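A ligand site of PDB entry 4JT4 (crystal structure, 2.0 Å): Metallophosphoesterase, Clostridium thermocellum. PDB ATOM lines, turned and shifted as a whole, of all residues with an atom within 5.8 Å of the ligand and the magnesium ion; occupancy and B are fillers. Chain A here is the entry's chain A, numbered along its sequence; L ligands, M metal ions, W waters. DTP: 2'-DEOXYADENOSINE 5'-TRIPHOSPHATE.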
ATOM      1  N   GLY A  16      -2.896 -16.067 -17.596  1.00  0.00           N
ATOM      2  CA  GLY A  16      -2.813 -16.957 -16.458  1.00  0.00           C
ATOM      3  C   GLY A  16      -4.106 -17.540 -15.980  1.00  0.00           C
ATOM      4  O   GLY A  16      -5.207 -16.968 -16.159  1.00  0.00           O
ATOM      5  N   SER A  17      -3.966 -18.702 -15.364  1.00  0.00           N
ATOM      6  CA  SER A  17      -5.088 -19.396 -14.750  1.00  0.00           C
ATOM      7  C   SER A  17      -5.854 -18.503 -13.806  1.00  0.00           C
ATOM      8  O   SER A  17      -5.313 -17.572 -13.234  1.00  0.00           O
ATOM      9  CB  SER A  17      -4.577 -20.596 -13.979  1.00  0.00           C
ATOM     10  OG  SER A  17      -5.644 -21.319 -13.430  1.00  0.00           O
ATOM     11  N   SER A  18      -7.140 -18.819 -13.644  1.00  0.00           N
ATOM     12  CA  SER A  18      -7.882 -18.323 -12.502  1.00  0.00           C
ATOM     13  C   SER A  18      -7.028 -18.630 -11.286  1.00  0.00           C
ATOM     14  O   SER A  18      -6.477 -19.724 -11.167  1.00  0.00           O
ATOM     15  CB  SER A  18      -9.222 -19.064 -12.379  1.00  0.00           C
ATOM     16  OG  SER A  18      -9.886 -18.688 -11.174  1.00  0.00           O
ATOM     17  N   GLY A  19      -6.888 -17.651 -10.403  1.00  0.00           N
ATOM     18  CA  GLY A  19      -6.109 -17.825  -9.198  1.00  0.00           C
ATOM     19  C   GLY A  19      -4.617 -17.559  -9.338  1.00  0.00           C
ATOM     20  O   GLY A  19      -3.887 -17.686  -8.358  1.00  0.00           O
ATOM     21  N   SER A  20      -4.162 -17.186 -10.539  1.00  0.00           N
ATOM     22  CA  SER A  20      -2.713 -17.020 -10.723  1.00  0.00           C
ATOM     23  C   SER A  20      -2.250 -15.649 -10.251  1.00  0.00           C
ATOM     24  O   SER A  20      -1.056 -15.385 -10.168  1.00  0.00           O
ATOM     25  CB  SER A  20      -2.289 -17.261 -12.171  1.00  0.00           C
ATOM     26  OG  SER A  20      -2.880 -16.286 -13.013  1.00  0.00           O
ATOM     27  N   GLY A  21      -3.193 -14.778  -9.936  1.00  0.00           N
ATOM     28  CA  GLY A  21      -2.880 -13.496  -9.345  1.00  0.00           C
ATOM     29  C   GLY A  21      -2.867 -12.346 -10.316  1.00  0.00           C
ATOM     30  O   GLY A  21      -2.270 -11.324 -10.015  1.00  0.00           O
ATOM     31  N   LYS A  22      -3.532 -12.479 -11.463  1.00  0.00           N
ATOM     32  CA  LYS A  22      -3.502 -11.425 -12.488  1.00  0.00           C
ATOM     33  C   LYS A  22      -4.032 -10.091 -12.009  1.00  0.00           C
ATOM     34  O   LYS A  22      -3.350  -9.048 -12.159  1.00  0.00           O
ATOM     35  CB  LYS A  22      -4.295 -11.833 -13.734  1.00  0.00           C
ATOM     36  CG  LYS A  22      -3.804 -13.127 -14.399  1.00  0.00           C
ATOM     37  CD  LYS A  22      -4.667 -13.462 -15.594  1.00  0.00           C
ATOM     38  CE  LYS A  22      -6.120 -13.782 -15.179  1.00  0.00           C
ATOM     39  NZ  LYS A  22      -6.217 -15.026 -14.332  1.00  0.00           N
ATOM     40  N   SER A  23      -5.232 -10.107 -11.442  1.00  0.00           N
ATOM     41  CA  SER A  23      -5.853  -8.857 -11.004  1.00  0.00           C
ATOM     42  C   SER A  23      -5.085  -8.231  -9.840  1.00  0.00           C
ATOM     43  O   SER A  23      -4.991  -7.007  -9.731  1.00  0.00           O
ATOM     44  CB  SER A  23      -7.326  -9.103 -10.590  1.00  0.00           C
ATOM     45  OG  SER A  23      -8.078  -9.708 -11.630  1.00  0.00           O
ATOM     46  N   THR A  24      -4.590  -9.090  -8.941  1.00  0.00           N
ATOM     47  CA  THR A  24      -3.673  -8.622  -7.879  1.00  0.00           C
ATOM     48  C   THR A  24      -2.467  -7.905  -8.510  1.00  0.00           C
ATOM     49  O   THR A  24      -2.129  -6.789  -8.135  1.00  0.00           O
ATOM     50  CB  THR A  24      -3.186  -9.790  -7.013  1.00  0.00           C
ATOM     51  OG1 THR A  24      -4.313 -10.502  -6.492  1.00  0.00           O
ATOM     52  CG2 THR A  24      -2.304  -9.290  -5.856  1.00  0.00           C
ATOM     53  N   PHE A  25      -1.841  -8.540  -9.499  1.00  0.00           N
ATOM     54  CA  PHE A  25      -0.674  -7.962 -10.190  1.00  0.00           C
ATOM     55  C   PHE A  25      -1.067  -6.639 -10.863  1.00  0.00           C
ATOM     56  O   PHE A  25      -0.365  -5.638 -10.727  1.00  0.00           O
ATOM     57  CB  PHE A  25      -0.149  -8.998 -11.203  1.00  0.00           C
ATOM     58  CG  PHE A  25       1.075  -8.587 -11.998  1.00  0.00           C
ATOM     59  CD1 PHE A  25       0.941  -7.934 -13.210  1.00  0.00           C
ATOM     60  CD2 PHE A  25       2.337  -8.967 -11.591  1.00  0.00           C
ATOM     61  CE1 PHE A  25       2.053  -7.615 -13.967  1.00  0.00           C
ATOM     62  CE2 PHE A  25       3.458  -8.661 -12.339  1.00  0.00           C
ATOM     63  CZ  PHE A  25       3.327  -7.981 -13.527  1.00  0.00           C
ATOM     64  N   ASP A  79      -7.036  -7.831 -18.440  1.00  0.00           N
ATOM     65  CA  ASP A  79      -7.008  -8.688 -17.267  1.00  0.00           C
ATOM     66  C   ASP A  79      -8.070  -9.741 -17.430  1.00  0.00           C
ATOM     67  O   ASP A  79      -9.237  -9.541 -17.065  1.00  0.00           O
ATOM     68  CB  ASP A  79      -7.202  -7.865 -15.981  1.00  0.00           C
ATOM     69  CG  ASP A  79      -7.304  -8.726 -14.737  1.00  0.00           C
ATOM     70  OD1 ASP A  79      -6.813  -9.875 -14.757  1.00  0.00           O
ATOM     71  OD2 ASP A  79      -7.880  -8.262 -13.732  1.00  0.00           O
ATOM     72  N   ALA A  80      -7.678 -10.858 -18.030  1.00  0.00           N
ATOM     73  CA  ALA A  80      -8.568 -11.967 -18.312  1.00  0.00           C
ATOM     74  C   ALA A  80      -7.660 -13.167 -18.350  1.00  0.00           C
ATOM     75  O   ALA A  80      -6.460 -13.015 -18.272  1.00  0.00           O
ATOM     76  CB  ALA A  80      -9.256 -11.764 -19.665  1.00  0.00           C
ATOM     77  N   THR A  81      -8.215 -14.360 -18.484  1.00  0.00           N
ATOM     78  CA  THR A  81      -7.364 -15.547 -18.409  1.00  0.00           C
ATOM     79  C   THR A  81      -6.406 -15.596 -19.600  1.00  0.00           C
ATOM     80  O   THR A  81      -5.217 -15.865 -19.419  1.00  0.00           O
ATOM     81  CB  THR A  81      -8.208 -16.839 -18.292  1.00  0.00           C
ATOM     82  OG1 THR A  81      -8.853 -17.114 -19.540  1.00  0.00           O
ATOM     83  CG2 THR A  81      -9.254 -16.670 -17.226  1.00  0.00           C
ATOM     84  N   ARG A 117      -4.480 -20.858  -3.708  1.00  0.00           N
ATOM     85  CA  ARG A 117      -5.013 -19.500  -3.548  1.00  0.00           C
ATOM     86  C   ARG A 117      -6.531 -19.423  -3.805  1.00  0.00           C
ATOM     87  O   ARG A 117      -7.255 -18.622  -3.187  1.00  0.00           O
ATOM     88  CB  ARG A 117      -4.319 -18.548  -4.519  1.00  0.00           C
ATOM     89  CG  ARG A 117      -2.804 -18.463  -4.401  1.00  0.00           C
ATOM     90  CD  ARG A 117      -2.300 -17.420  -5.348  1.00  0.00           C
ATOM     91  NE  ARG A 117      -0.867 -17.186  -5.199  1.00  0.00           N
ATOM     92  CZ  ARG A 117      -0.131 -16.554  -6.103  1.00  0.00           C
ATOM     93  NH1 ARG A 117      -0.683 -16.105  -7.220  1.00  0.00           N
ATOM     94  NH2 ARG A 117       1.153 -16.391  -5.893  1.00  0.00           N
ATOM     95  N   ASN A 118      -7.006 -20.252  -4.726  1.00  0.00           N
ATOM     96  CA  ASN A 118      -8.431 -20.307  -5.073  1.00  0.00           C
ATOM     97  C   ASN A 118      -9.318 -20.588  -3.847  1.00  0.00           C
ATOM     98  O   ASN A 118     -10.306 -19.903  -3.618  1.00  0.00           O
ATOM     99  CB  ASN A 118      -8.659 -21.394  -6.131  1.00  0.00           C
ATOM    100  CG  ASN A 118     -10.140 -21.572  -6.495  1.00  0.00           C
ATOM    101  OD1 ASN A 118     -10.835 -20.622  -6.835  1.00  0.00           O
ATOM    102  ND2 ASN A 118     -10.607 -22.821  -6.444  1.00  0.00           N
ATOM    103  N   ASN A 120      -8.984 -20.009  -0.910  1.00  0.00           N
ATOM    104  CA  ASN A 120      -8.972 -18.947   0.085  1.00  0.00           C
ATOM    105  C   ASN A 120      -9.509 -17.601  -0.393  1.00  0.00           C
ATOM    106  O   ASN A 120      -9.483 -16.630   0.357  1.00  0.00           O
ATOM    107  CB  ASN A 120      -7.590 -18.802   0.706  1.00  0.00           C
ATOM    108  CG  ASN A 120      -7.166 -20.051   1.471  1.00  0.00           C
ATOM    109  OD1 ASN A 120      -7.727 -20.357   2.510  1.00  0.00           O
ATOM    110  ND2 ASN A 120      -6.178 -20.767   0.954  1.00  0.00           N
ATOM    111  N   ARG A 121      -9.991 -17.541  -1.635  1.00  0.00           N
ATOM    112  CA  ARG A 121     -10.574 -16.313  -2.180  1.00  0.00           C
ATOM    113  C   ARG A 121     -11.860 -15.908  -1.494  1.00  0.00           C
ATOM    114  O   ARG A 121     -12.684 -16.745  -1.153  1.00  0.00           O
ATOM    115  CB  ARG A 121     -10.898 -16.482  -3.676  1.00  0.00           C
ATOM    116  CG  ARG A 121      -9.678 -16.825  -4.525  1.00  0.00           C
ATOM    117  CD  ARG A 121     -10.048 -16.797  -6.004  1.00  0.00           C
ATOM    118  NE  ARG A 121     -10.476 -15.472  -6.435  1.00  0.00           N
ATOM    119  CZ  ARG A 121     -10.493 -15.081  -7.703  1.00  0.00           C
ATOM    120  NH1 ARG A 121     -10.105 -15.936  -8.651  1.00  0.00           N
ATOM    121  NH2 ARG A 121     -10.902 -13.865  -8.028  1.00  0.00           N
ATOM    122  N   THR A 122     -12.057 -14.601  -1.342  1.00  0.00           N
ATOM    123  CA  THR A 122     -13.280 -14.080  -0.741  1.00  0.00           C
ATOM    124  C   THR A 122     -14.299 -13.674  -1.782  1.00  0.00           C
ATOM    125  O   THR A 122     -15.512 -13.746  -1.536  1.00  0.00           O
ATOM    126  CB  THR A 122     -12.998 -12.860   0.184  1.00  0.00           C
ATOM    127  OG1 THR A 122     -12.129 -11.933  -0.477  1.00  0.00           O
ATOM    128  CG2 THR A 122     -12.343 -13.314   1.462  1.00  0.00           C
ATOM    129  N   ASP A 123     -13.826 -13.248  -2.946  1.00  0.00           N
ATOM    130  CA  ASP A 123     -14.729 -12.723  -3.991  1.00  0.00           C
ATOM    131  C   ASP A 123     -15.526 -13.830  -4.667  1.00  0.00           C
ATOM    132  O   ASP A 123     -16.753 -13.806  -4.670  1.00  0.00           O
ATOM    133  CB  ASP A 123     -13.953 -11.904  -5.041  1.00  0.00           C
ATOM    134  CG  ASP A 123     -12.619 -12.540  -5.426  1.00  0.00           C
ATOM    135  OD1 ASP A 123     -12.224 -13.584  -4.865  1.00  0.00           O
ATOM    136  OD2 ASP A 123     -11.939 -11.955  -6.306  1.00  0.00           O
ATOM    137  N   ARG A 124     -14.821 -14.785  -5.256  1.00  0.00           N
ATOM    138  CA  ARG A 124     -15.460 -15.915  -5.915  1.00  0.00           C
ATOM    139  C   ARG A 124     -14.419 -17.006  -6.050  1.00  0.00           C
ATOM    140  O   ARG A 124     -13.225 -16.752  -5.897  1.00  0.00           O
ATOM    141  CB  ARG A 124     -15.951 -15.508  -7.301  1.00  0.00           C
ATOM    142  CG  ARG A 124     -14.847 -14.995  -8.203  1.00  0.00           C
ATOM    143  CD  ARG A 124     -15.384 -14.325  -9.461  1.00  0.00           C
ATOM    144  NE  ARG A 124     -14.303 -13.628 -10.135  1.00  0.00           N
ATOM    145  CZ  ARG A 124     -13.394 -14.217 -10.906  1.00  0.00           C
ATOM    146  NH1 ARG A 124     -13.441 -15.525 -11.117  1.00  0.00           N
ATOM    147  NH2 ARG A 124     -12.439 -13.498 -11.466  1.00  0.00           N
ATOM    148  N   VAL A 126     -13.570 -20.991  -8.190  1.00  0.00           N
ATOM    149  CA  VAL A 126     -13.957 -21.903  -9.254  1.00  0.00           C
ATOM    150  C   VAL A 126     -13.643 -23.335  -8.828  1.00  0.00           C
ATOM    151  O   VAL A 126     -12.886 -23.563  -7.883  1.00  0.00           O
ATOM    152  CB  VAL A 126     -13.205 -21.550 -10.591  1.00  0.00           C
ATOM    153  CG1 VAL A 126     -13.477 -20.116 -10.997  1.00  0.00           C
ATOM    154  CG2 VAL A 126     -11.706 -21.763 -10.433  1.00  0.00           C
ATOM    155  N   PRO A 159       6.221 -17.380  -7.833  1.00  0.00           N
ATOM    156  CA  PRO A 159       5.707 -16.216  -7.094  1.00  0.00           C
ATOM    157  C   PRO A 159       6.789 -15.186  -6.783  1.00  0.00           C
ATOM    158  O   PRO A 159       6.535 -13.992  -6.799  1.00  0.00           O
ATOM    159  CB  PRO A 159       5.181 -16.846  -5.807  1.00  0.00           C
ATOM    160  CG  PRO A 159       4.713 -18.182  -6.233  1.00  0.00           C
ATOM    161  CD  PRO A 159       5.723 -18.638  -7.259  1.00  0.00           C
ATOM    162  N   VAL A 162       7.320 -13.110  -9.778  1.00  0.00           N
ATOM    163  CA  VAL A 162       6.180 -12.201  -9.931  1.00  0.00           C
ATOM    164  C   VAL A 162       6.329 -10.992  -9.027  1.00  0.00           C
ATOM    165  O   VAL A 162       6.191  -9.845  -9.463  1.00  0.00           O
ATOM    166  CB  VAL A 162       4.831 -12.889  -9.598  1.00  0.00           C
ATOM    167  CG1 VAL A 162       3.735 -11.839  -9.480  1.00  0.00           C
ATOM    168  CG2 VAL A 162       4.484 -13.961 -10.644  1.00  0.00           C
ATOM    169  N   GLU A 163       6.593 -11.274  -7.744  1.00  0.00           N
ATOM    170  CA  GLU A 163       6.862 -10.247  -6.735  1.00  0.00           C
ATOM    171  C   GLU A 163       7.944  -9.270  -7.148  1.00  0.00           C
ATOM    172  O   GLU A 163       7.795  -8.069  -6.940  1.00  0.00           O
ATOM    173  CB  GLU A 163       7.318 -10.934  -5.428  1.00  0.00           C
ATOM    174  CG  GLU A 163       6.284 -10.914  -4.322  1.00  0.00           C
ATOM    175  CD  GLU A 163       6.174  -9.568  -3.650  1.00  0.00           C
ATOM    176  OE1 GLU A 163       7.227  -9.026  -3.245  1.00  0.00           O
ATOM    177  OE2 GLU A 163       5.042  -9.043  -3.533  1.00  0.00           O
HETATM  178  PG  DTP L   1      -9.299 -14.741 -12.001  1.00  0.00           P
HETATM  179  O1G DTP L   1     -10.205 -15.789 -11.457  1.00  0.00           O
HETATM  180  O2G DTP L   1      -8.759 -15.120 -13.368  1.00  0.00           O
HETATM  181  O3G DTP L   1      -9.772 -13.298 -11.921  1.00  0.00           O
HETATM  182  PB  DTP L   1      -6.785 -13.840 -10.905  1.00  0.00           P
HETATM  183  O1B DTP L   1      -5.655 -14.419 -11.736  1.00  0.00           O
HETATM  184  O2B DTP L   1      -7.279 -12.438 -11.093  1.00  0.00           O
HETATM  185  O3B DTP L   1      -8.016 -14.881 -10.995  1.00  0.00           O
HETATM  186  PA  DTP L   1      -6.418 -12.872  -8.238  1.00  0.00           P
HETATM  187  O1A DTP L   1      -5.510 -11.696  -8.451  1.00  0.00           O
HETATM  188  O2A DTP L   1      -7.885 -12.619  -8.047  1.00  0.00           O
HETATM  189  O3A DTP L   1      -6.261 -14.005  -9.385  1.00  0.00           O
HETATM  190  O5' DTP L   1      -5.860 -13.699  -6.961  1.00  0.00           O
HETATM  191  C5' DTP L   1      -6.522 -14.878  -6.507  1.00  0.00           C
HETATM  192  C4' DTP L   1      -6.279 -15.037  -4.995  1.00  0.00           C
HETATM  193  O4' DTP L   1      -4.882 -15.194  -4.708  1.00  0.00           O
HETATM  194  C3' DTP L   1      -6.725 -13.804  -4.227  1.00  0.00           C
HETATM  195  O3' DTP L   1      -7.334 -14.280  -3.019  1.00  0.00           O
HETATM  196  C2' DTP L   1      -5.453 -13.036  -3.892  1.00  0.00           C
HETATM  197  C1' DTP L   1      -4.412 -14.149  -3.868  1.00  0.00           C
HETATM  198  N9  DTP L   1      -3.077 -13.713  -4.357  1.00  0.00           N
HETATM  199  C8  DTP L   1      -2.821 -13.086  -5.523  1.00  0.00           C
HETATM  200  N7  DTP L   1      -1.494 -12.849  -5.666  1.00  0.00           N
HETATM  201  C5  DTP L   1      -0.877 -13.331  -4.584  1.00  0.00           C
HETATM  202  C6  DTP L   1       0.525 -13.405  -4.093  1.00  0.00           C
HETATM  203  N6  DTP L   1       1.550 -12.907  -4.815  1.00  0.00           N
HETATM  204  N1  DTP L   1       0.748 -13.996  -2.894  1.00  0.00           N
HETATM  205  C2  DTP L   1      -0.259 -14.508  -2.164  1.00  0.00           C
HETATM  206  N3  DTP L   1      -1.552 -14.474  -2.539  1.00  0.00           N
HETATM  207  C4  DTP L   1      -1.918 -13.898  -3.720  1.00  0.00           C
HETATM  208 MG    MG M   1      -9.016 -11.554 -11.691  1.00  0.00          MG
HETATM  209  O   HOH W   1     -10.758 -10.711 -12.346  1.00  0.00           O
HETATM  210  O   HOH W   2       4.251 -13.369  -5.958  1.00  0.00           O
HETATM  211  O   HOH W   3       0.400 -11.688  -7.863  1.00  0.00           O
HETATM  212  O   HOH W   4      -9.612 -11.502  -9.602  1.00  0.00           O
HETATM  213  O   HOH W   5     -10.605 -16.807 -14.474  1.00  0.00           O
HETATM  214  O   HOH W   6      -3.099 -14.212   0.087  1.00  0.00           O
HETATM  215  O   HOH W   7      -9.084 -11.525  -5.872  1.00  0.00           O
HETATM  216  O   HOH W   8      -8.556 -11.651 -13.766  1.00  0.00           O
HETATM  217  O   HOH W   9      -6.428 -16.657  -1.898  1.00  0.00           O
HETATM  218  O   HOH W  10      -9.653 -13.579 -15.221  1.00  0.00           O
HETATM  219  O   HOH W  11       3.496 -10.812  -5.722  1.00  0.00           O
HETATM  220  O   HOH W  12      -9.957 -12.737  -2.191  1.00  0.00           O
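An oxygen (O1A) of the ligand lies within hydrogen-bond range of the backbone NH (N) of Ser 23, 3.4 Å away.
The backbone NH (N) of Thr 24 sits at hydrogen-bond distance from an oxygen (O1A) of the ligand.
The side-chain hydroxyl (OG1) of Thr 24 is in hydrogen-bond range of an oxygen (O1A) of the ligand (2.6 Å).
An oxygen (O1G) of the ligand lies within salt-bridge range of the guanidinium group of Arg 124, 3.2 Å away.
The backbone NH (N) of Lys 22 sits at hydrogen-bond distance from an oxygen (O1B) of the ligand (2.9 Å).
The side-chain amino group of Lys 22 is in salt-bridge range of an oxygen (O2G) of the ligand, at 2.7 Å.
NH1 of Arg 121 is in salt-bridge range of O1G of the ligand (2.8 Å).
O1G of the ligand sits at hydrogen-bond distance from OG of Ser 18 (2.9 Å).
An oxygen (O3B) of the ligand sits at hydrogen-bond distance from the backbone NH (N) of Gly 19 (3.0 Å).
O1B of the ligand lies within hydrogen-bond range of N of Gly 21.
The backbone NH of Ser 20 lies within hydrogen-bond range of an oxygen (O1B) of the ligand (3.4 Å).
The side-chain hydroxyl (OG) of Ser 23 sits close to the side-chain carboxylate (OD2) of Asp 79, 2.6 Å away.
The guanidinium group (NE) of Arg 121 lies within hydrogen-bond range of the backbone carbonyl oxygen (O) of Arg 124 (3.1 Å).
NZ of Lys 22 is in hydrogen-bond range of O of Ser 17 (2.9 Å).
NZ of Lys 22 lies within hydrogen-bond range of O of Gly 16 (2.9 Å).
OD2 of Asp 123 is in salt-bridge range of NH2 of Arg 121, 2.8 Å away.
The backbone carbonyl oxygen (O) of Ser 20 sits at hydrogen-bond distance from the guanidinium group (NH1) of Arg 117 (3.1 Å).
OG of Ser 20 sits at hydrogen-bond distance from O of Ser 17, at 2.8 Å.
Residues that only touch the ligand: Arg 117 and Ser 17.
The nearest printed residue that does not touch the ligand is Thr 81 (4.2 Å).
NH2 of Arg 124 touches the magnesium ion, at 3.9 Å.
Two residues have an atom within 4 Å of the magnesium ion: Ser 23 and Arg 124.
O3G of the ligand is bound to the magnesium ion, 1.9 Å away.
An oxygen (O2B) of the ligand is bound to the magnesium ion, at 2.0 Å.
The magnesium ion is bound by water W1, 2.0 Å away.
OG of Ser 23 binds the magnesium ion (2.1 Å).
Water W8 is bound to the magnesium ion, at 2.1 Å.
Water W4 binds the magnesium ion (2.2 Å).
Water W8 bridges OD1 of Asp 79 (2.7 Å) and O2G of the ligand (3.5 Å).
Water W4 bridges an oxygen (O2A) of the ligand (2.6 Å) and the guanidinium group of Arg 121 (3.1 Å).
Water W9 bridges O of Arg 117 (2.5 Å) and O3' of the ligand (2.8 Å).
Water W11 bridges a nitrogen (N6) of the ligand (3.0 Å) and the side-chain carboxylate (OE2) of Glu 163 (3.2 Å).
Water W3 lies within hydrogen-bond range of N7 of the ligand (3.1 Å) and O of Gly 21 (3.4 Å).
Water W12 bridges OG1 of Thr 122 (2.9 Å) and O3' of the ligand (3.2 Å).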
